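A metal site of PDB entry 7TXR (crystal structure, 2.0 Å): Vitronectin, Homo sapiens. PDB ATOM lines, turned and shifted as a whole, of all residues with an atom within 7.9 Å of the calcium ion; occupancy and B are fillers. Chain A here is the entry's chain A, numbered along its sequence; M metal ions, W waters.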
ATOM      1  N   PHE A   9      12.477 -18.315 -31.217  1.00  0.00           N
ATOM      2  CA  PHE A   9      13.457 -18.050 -30.120  1.00  0.00           C
ATOM      3  C   PHE A   9      14.009 -19.368 -29.609  1.00  0.00           C
ATOM      4  O   PHE A   9      13.349 -20.411 -29.797  1.00  0.00           O
ATOM      5  CB  PHE A   9      12.821 -17.165 -29.045  1.00  0.00           C
ATOM      6  CG  PHE A   9      12.665 -15.734 -29.485  1.00  0.00           C
ATOM      7  CD1 PHE A   9      13.692 -14.824 -29.295  1.00  0.00           C
ATOM      8  CD2 PHE A   9      11.516 -15.300 -30.127  1.00  0.00           C
ATOM      9  CE1 PHE A   9      13.568 -13.515 -29.718  1.00  0.00           C
ATOM     10  CE2 PHE A   9      11.386 -13.979 -30.507  1.00  0.00           C
ATOM     11  CZ  PHE A   9      12.429 -13.099 -30.353  1.00  0.00           C
ATOM     12  N   ASP A  10      15.195 -19.300 -28.986  1.00  0.00           N
ATOM     13  CA  ASP A  10      15.946 -20.458 -28.430  1.00  0.00           C
ATOM     14  C   ASP A  10      15.686 -20.587 -26.921  1.00  0.00           C
ATOM     15  O   ASP A  10      15.708 -21.700 -26.403  1.00  0.00           O
ATOM     16  CB  ASP A  10      17.435 -20.284 -28.666  1.00  0.00           C
ATOM     17  CG  ASP A  10      17.844 -20.365 -30.144  1.00  0.00           C
ATOM     18  OD1 ASP A  10      17.056 -20.868 -30.965  1.00  0.00           O
ATOM     19  OD2 ASP A  10      18.943 -19.850 -30.454  1.00  0.00           O
ATOM     20  N   ALA A  11      15.585 -19.471 -26.210  1.00  0.00           N
ATOM     21  CA  ALA A  11      15.458 -19.448 -24.731  1.00  0.00           C
ATOM     22  C   ALA A  11      15.051 -18.050 -24.270  1.00  0.00           C
ATOM     23  O   ALA A  11      15.290 -17.036 -25.020  1.00  0.00           O
ATOM     24  CB  ALA A  11      16.766 -19.861 -24.096  1.00  0.00           C
ATOM     25  N   PHE A  12      14.462 -17.988 -23.068  1.00  0.00           N
ATOM     26  CA  PHE A  12      14.085 -16.738 -22.363  1.00  0.00           C
ATOM     27  C   PHE A  12      14.420 -16.900 -20.895  1.00  0.00           C
ATOM     28  O   PHE A  12      14.261 -18.013 -20.370  1.00  0.00           O
ATOM     29  CB  PHE A  12      12.590 -16.474 -22.463  1.00  0.00           C
ATOM     30  CG  PHE A  12      12.064 -16.098 -23.819  1.00  0.00           C
ATOM     31  CD1 PHE A  12      11.663 -17.073 -24.717  1.00  0.00           C
ATOM     32  CD2 PHE A  12      12.033 -14.771 -24.218  1.00  0.00           C
ATOM     33  CE1 PHE A  12      11.197 -16.717 -25.977  1.00  0.00           C
ATOM     34  CE2 PHE A  12      11.516 -14.427 -25.462  1.00  0.00           C
ATOM     35  CZ  PHE A  12      11.140 -15.406 -26.347  1.00  0.00           C
ATOM     36  N   PHE A  23      16.885 -15.082 -26.216  1.00  0.00           N
ATOM     37  CA  PHE A  23      18.059 -15.617 -26.938  1.00  0.00           C
ATOM     38  C   PHE A  23      17.593 -16.156 -28.290  1.00  0.00           C
ATOM     39  O   PHE A  23      16.584 -16.861 -28.356  1.00  0.00           O
ATOM     40  CB  PHE A  23      18.777 -16.699 -26.131  1.00  0.00           C
ATOM     41  CG  PHE A  23      19.303 -16.190 -24.824  1.00  0.00           C
ATOM     42  CD1 PHE A  23      18.512 -16.217 -23.686  1.00  0.00           C
ATOM     43  CD2 PHE A  23      20.564 -15.615 -24.751  1.00  0.00           C
ATOM     44  CE1 PHE A  23      18.985 -15.699 -22.491  1.00  0.00           C
ATOM     45  CE2 PHE A  23      21.037 -15.097 -23.555  1.00  0.00           C
ATOM     46  CZ  PHE A  23      20.260 -15.173 -22.412  1.00  0.00           C
ATOM     47  N   ILE A  54      21.960 -20.842 -27.088  1.00  0.00           N
ATOM     48  CA  ILE A  54      21.724 -21.495 -25.777  1.00  0.00           C
ATOM     49  C   ILE A  54      20.400 -22.289 -25.846  1.00  0.00           C
ATOM     50  O   ILE A  54      19.506 -21.936 -26.642  1.00  0.00           O
ATOM     51  CB  ILE A  54      21.877 -20.530 -24.592  1.00  0.00           C
ATOM     52  CG1 ILE A  54      20.604 -19.748 -24.307  1.00  0.00           C
ATOM     53  CG2 ILE A  54      23.077 -19.577 -24.720  1.00  0.00           C
ATOM     54  CD1 ILE A  54      20.511 -19.327 -22.884  1.00  0.00           C
ATOM     55  N   ASP A  55      20.343 -23.367 -25.077  1.00  0.00           N
ATOM     56  CA  ASP A  55      19.232 -24.364 -25.053  1.00  0.00           C
ATOM     57  C   ASP A  55      18.023 -23.803 -24.302  1.00  0.00           C
ATOM     58  O   ASP A  55      16.912 -23.835 -24.828  1.00  0.00           O
ATOM     59  CB  ASP A  55      19.675 -25.660 -24.374  1.00  0.00           C
ATOM     60  CG  ASP A  55      20.631 -26.473 -25.228  1.00  0.00           C
ATOM     61  OD1 ASP A  55      20.834 -26.069 -26.388  1.00  0.00           O
ATOM     62  OD2 ASP A  55      21.185 -27.477 -24.716  1.00  0.00           O
ATOM     63  N   ALA A  56      18.274 -23.315 -23.104  1.00  0.00           N
ATOM     64  CA  ALA A  56      17.240 -22.902 -22.144  1.00  0.00           C
ATOM     65  C   ALA A  56      17.844 -21.942 -21.162  1.00  0.00           C
ATOM     66  O   ALA A  56      19.079 -21.971 -21.010  1.00  0.00           O
ATOM     67  CB  ALA A  56      16.691 -24.122 -21.406  1.00  0.00           C
ATOM     68  N   ALA A  57      16.986 -21.232 -20.429  1.00  0.00           N
ATOM     69  CA  ALA A  57      17.416 -20.305 -19.370  1.00  0.00           C
ATOM     70  C   ALA A  57      16.312 -20.198 -18.336  1.00  0.00           C
ATOM     71  O   ALA A  57      15.139 -20.424 -18.688  1.00  0.00           O
ATOM     72  CB  ALA A  57      17.735 -18.965 -19.989  1.00  0.00           C
ATOM     73  N   PHE A  70      21.772 -22.730 -20.131  1.00  0.00           N
ATOM     74  CA  PHE A  70      22.044 -24.162 -20.390  1.00  0.00           C
ATOM     75  C   PHE A  70      22.454 -24.308 -21.841  1.00  0.00           C
ATOM     76  O   PHE A  70      21.806 -23.698 -22.719  1.00  0.00           O
ATOM     77  CB  PHE A  70      20.808 -25.015 -20.074  1.00  0.00           C
ATOM     78  CG  PHE A  70      20.428 -24.925 -18.633  1.00  0.00           C
ATOM     79  CD1 PHE A  70      19.733 -23.835 -18.131  1.00  0.00           C
ATOM     80  CD2 PHE A  70      20.774 -25.944 -17.759  1.00  0.00           C
ATOM     81  CE1 PHE A  70      19.431 -23.747 -16.778  1.00  0.00           C
ATOM     82  CE2 PHE A  70      20.490 -25.847 -16.407  1.00  0.00           C
ATOM     83  CZ  PHE A  70      19.812 -24.747 -15.919  1.00  0.00           C
ATOM     84  N   ASN A 101      20.765 -31.334 -22.922  1.00  0.00           N
ATOM     85  CA  ASN A 101      20.126 -30.846 -24.172  1.00  0.00           C
ATOM     86  C   ASN A 101      18.649 -30.534 -23.896  1.00  0.00           C
ATOM     87  O   ASN A 101      17.784 -30.975 -24.691  1.00  0.00           O
ATOM     88  CB  ASN A 101      20.321 -31.844 -25.309  1.00  0.00           C
ATOM     89  CG  ASN A 101      21.782 -32.049 -25.666  1.00  0.00           C
ATOM     90  OD1 ASN A 101      22.447 -31.089 -26.061  1.00  0.00           O
ATOM     91  ND2 ASN A 101      22.264 -33.280 -25.582  1.00  0.00           N
ATOM     92  N   VAL A 102      18.364 -29.814 -22.811  1.00  0.00           N
ATOM     93  CA  VAL A 102      16.947 -29.463 -22.502  1.00  0.00           C
ATOM     94  C   VAL A 102      16.435 -28.506 -23.597  1.00  0.00           C
ATOM     95  O   VAL A 102      17.286 -27.820 -24.232  1.00  0.00           O
ATOM     96  CB  VAL A 102      16.791 -28.883 -21.087  1.00  0.00           C
ATOM     97  CG1 VAL A 102      17.059 -29.937 -20.040  1.00  0.00           C
ATOM     98  CG2 VAL A 102      17.649 -27.656 -20.860  1.00  0.00           C
ATOM     99  N   ASP A 103      15.122 -28.461 -23.794  1.00  0.00           N
ATOM    100  CA  ASP A 103      14.459 -27.597 -24.793  1.00  0.00           C
ATOM    101  C   ASP A 103      14.225 -26.218 -24.176  1.00  0.00           C
ATOM    102  O   ASP A 103      14.332 -25.252 -24.901  1.00  0.00           O
ATOM    103  CB  ASP A 103      13.157 -28.164 -25.339  1.00  0.00           C
ATOM    104  CG  ASP A 103      13.314 -29.413 -26.190  1.00  0.00           C
ATOM    105  OD1 ASP A 103      14.371 -29.556 -26.805  1.00  0.00           O
ATOM    106  OD2 ASP A 103      12.338 -30.221 -26.238  1.00  0.00           O
ATOM    107  N   ALA A 104      13.855 -26.155 -22.899  1.00  0.00           N
ATOM    108  CA  ALA A 104      13.356 -24.936 -22.246  1.00  0.00           C
ATOM    109  C   ALA A 104      13.365 -25.145 -20.751  1.00  0.00           C
ATOM    110  O   ALA A 104      13.422 -26.284 -20.292  1.00  0.00           O
ATOM    111  CB  ALA A 104      11.984 -24.627 -22.740  1.00  0.00           C
ATOM    112  N   ALA A 105      13.200 -24.056 -20.017  1.00  0.00           N
ATOM    113  CA  ALA A 105      13.129 -24.075 -18.549  1.00  0.00           C
ATOM    114  C   ALA A 105      12.386 -22.833 -18.084  1.00  0.00           C
ATOM    115  O   ALA A 105      12.390 -21.825 -18.817  1.00  0.00           O
ATOM    116  CB  ALA A 105      14.521 -24.120 -17.965  1.00  0.00           C
ATOM    117  N   PHE A 122      12.055 -28.715 -19.656  1.00  0.00           N
ATOM    118  CA  PHE A 122      11.249 -29.304 -20.740  1.00  0.00           C
ATOM    119  C   PHE A 122      12.198 -29.922 -21.744  1.00  0.00           C
ATOM    120  O   PHE A 122      13.158 -29.259 -22.165  1.00  0.00           O
ATOM    121  CB  PHE A 122      10.298 -28.261 -21.311  1.00  0.00           C
ATOM    122  CG  PHE A 122       9.402 -27.634 -20.267  1.00  0.00           C
ATOM    123  CD1 PHE A 122       9.857 -26.576 -19.496  1.00  0.00           C
ATOM    124  CD2 PHE A 122       8.117 -28.124 -20.040  1.00  0.00           C
ATOM    125  CE1 PHE A 122       9.040 -26.015 -18.527  1.00  0.00           C
ATOM    126  CE2 PHE A 122       7.305 -27.552 -19.078  1.00  0.00           C
ATOM    127  CZ  PHE A 122       7.758 -26.494 -18.335  1.00  0.00           C
ATOM    128  N   VAL A 156       8.387 -27.802 -26.896  1.00  0.00           N
ATOM    129  CA  VAL A 156       8.511 -26.317 -26.845  1.00  0.00           C
ATOM    130  C   VAL A 156       9.959 -25.944 -27.181  1.00  0.00           C
ATOM    131  O   VAL A 156      10.881 -26.766 -27.034  1.00  0.00           O
ATOM    132  CB  VAL A 156       8.039 -25.743 -25.487  1.00  0.00           C
ATOM    133  CG1 VAL A 156       6.599 -26.133 -25.215  1.00  0.00           C
ATOM    134  CG2 VAL A 156       8.930 -26.155 -24.331  1.00  0.00           C
ATOM    135  N   ASP A 157      10.146 -24.713 -27.669  1.00  0.00           N
ATOM    136  CA  ASP A 157      11.466 -24.144 -28.002  1.00  0.00           C
ATOM    137  C   ASP A 157      12.047 -23.424 -26.791  1.00  0.00           C
ATOM    138  O   ASP A 157      13.274 -23.358 -26.693  1.00  0.00           O
ATOM    139  CB  ASP A 157      11.345 -23.158 -29.162  1.00  0.00           C
ATOM    140  CG  ASP A 157      10.921 -23.814 -30.455  1.00  0.00           C
ATOM    141  OD1 ASP A 157      11.096 -25.038 -30.613  1.00  0.00           O
ATOM    142  OD2 ASP A 157      10.402 -23.105 -31.308  1.00  0.00           O
ATOM    143  N   ALA A 158      11.177 -22.878 -25.941  1.00  0.00           N
ATOM    144  CA  ALA A 158      11.540 -21.930 -24.900  1.00  0.00           C
ATOM    145  C   ALA A 158      10.330 -21.680 -24.014  1.00  0.00           C
ATOM    146  O   ALA A 158       9.187 -21.983 -24.426  1.00  0.00           O
ATOM    147  CB  ALA A 158      12.047 -20.626 -25.520  1.00  0.00           C
ATOM    148  N   ALA A 159      10.582 -21.152 -22.823  1.00  0.00           N
ATOM    149  CA  ALA A 159       9.547 -20.902 -21.824  1.00  0.00           C
ATOM    150  C   ALA A 159      10.020 -19.767 -20.932  1.00  0.00           C
ATOM    151  O   ALA A 159      11.272 -19.553 -20.796  1.00  0.00           O
ATOM    152  CB  ALA A 159       9.256 -22.178 -21.028  1.00  0.00           C
ATOM    153  N   PHE A 169       6.833 -21.191 -25.913  1.00  0.00           N
ATOM    154  CA  PHE A 169       7.180 -20.708 -27.283  1.00  0.00           C
ATOM    155  C   PHE A 169       7.413 -21.931 -28.165  1.00  0.00           C
ATOM    156  O   PHE A 169       8.114 -22.875 -27.750  1.00  0.00           O
ATOM    157  CB  PHE A 169       8.350 -19.732 -27.210  1.00  0.00           C
ATOM    158  CG  PHE A 169       8.113 -18.562 -26.287  1.00  0.00           C
ATOM    159  CD1 PHE A 169       8.376 -18.661 -24.941  1.00  0.00           C
ATOM    160  CD2 PHE A 169       7.641 -17.370 -26.783  1.00  0.00           C
ATOM    161  CE1 PHE A 169       8.173 -17.580 -24.106  1.00  0.00           C
ATOM    162  CE2 PHE A 169       7.399 -16.303 -25.940  1.00  0.00           C
ATOM    163  CZ  PHE A 169       7.666 -16.408 -24.587  1.00  0.00           C
HETATM  164 CA    CA M   1      15.467 -24.053 -26.563  1.00  0.00          CA
HETATM  165  O   HOH W   1      14.924 -25.136 -28.477  1.00  0.00           O
HETATM  166  O   HOH W   2      16.755 -26.060 -26.730  1.00  0.00           O
HETATM  167  O   HOH W   3      17.424 -23.484 -27.992  1.00  0.00           O
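Four residues have an atom within 4 Å of the calcium ion: Asp 10, Asp 55, Asp 103 and Asp 157.
The backbone NH of Asp 10 lies within hydrogen-bond range of the backbone carbonyl oxygen of Phe 23.
N of Asp 157 is in hydrogen-bond range of O of Phe 169, 2.7 Å away.
The backbone NH (N) of Asp 103 lies within hydrogen-bond range of the backbone carbonyl oxygen (O) of Phe 122 (2.7 Å).
The backbone NH (N) of Asp 55 sits at hydrogen-bond distance from the backbone carbonyl oxygen (O) of Phe 70 (2.8 Å).
The calcium ion is bound by water W1 (2.3 Å), the backbone carbonyl oxygen (O) of Asp 55 (2.3 Å), the backbone carbonyl oxygen (O) of Asp 157 (2.3 Å), the backbone carbonyl oxygen (O) of Asp 103 (2.3 Å), the backbone carbonyl oxygen (O) of Asp 10 (2.4 Å), water W2 (2.4 Å) and water W3 (2.5 Å).
The calcium ion has seven donor atoms within binding distance.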
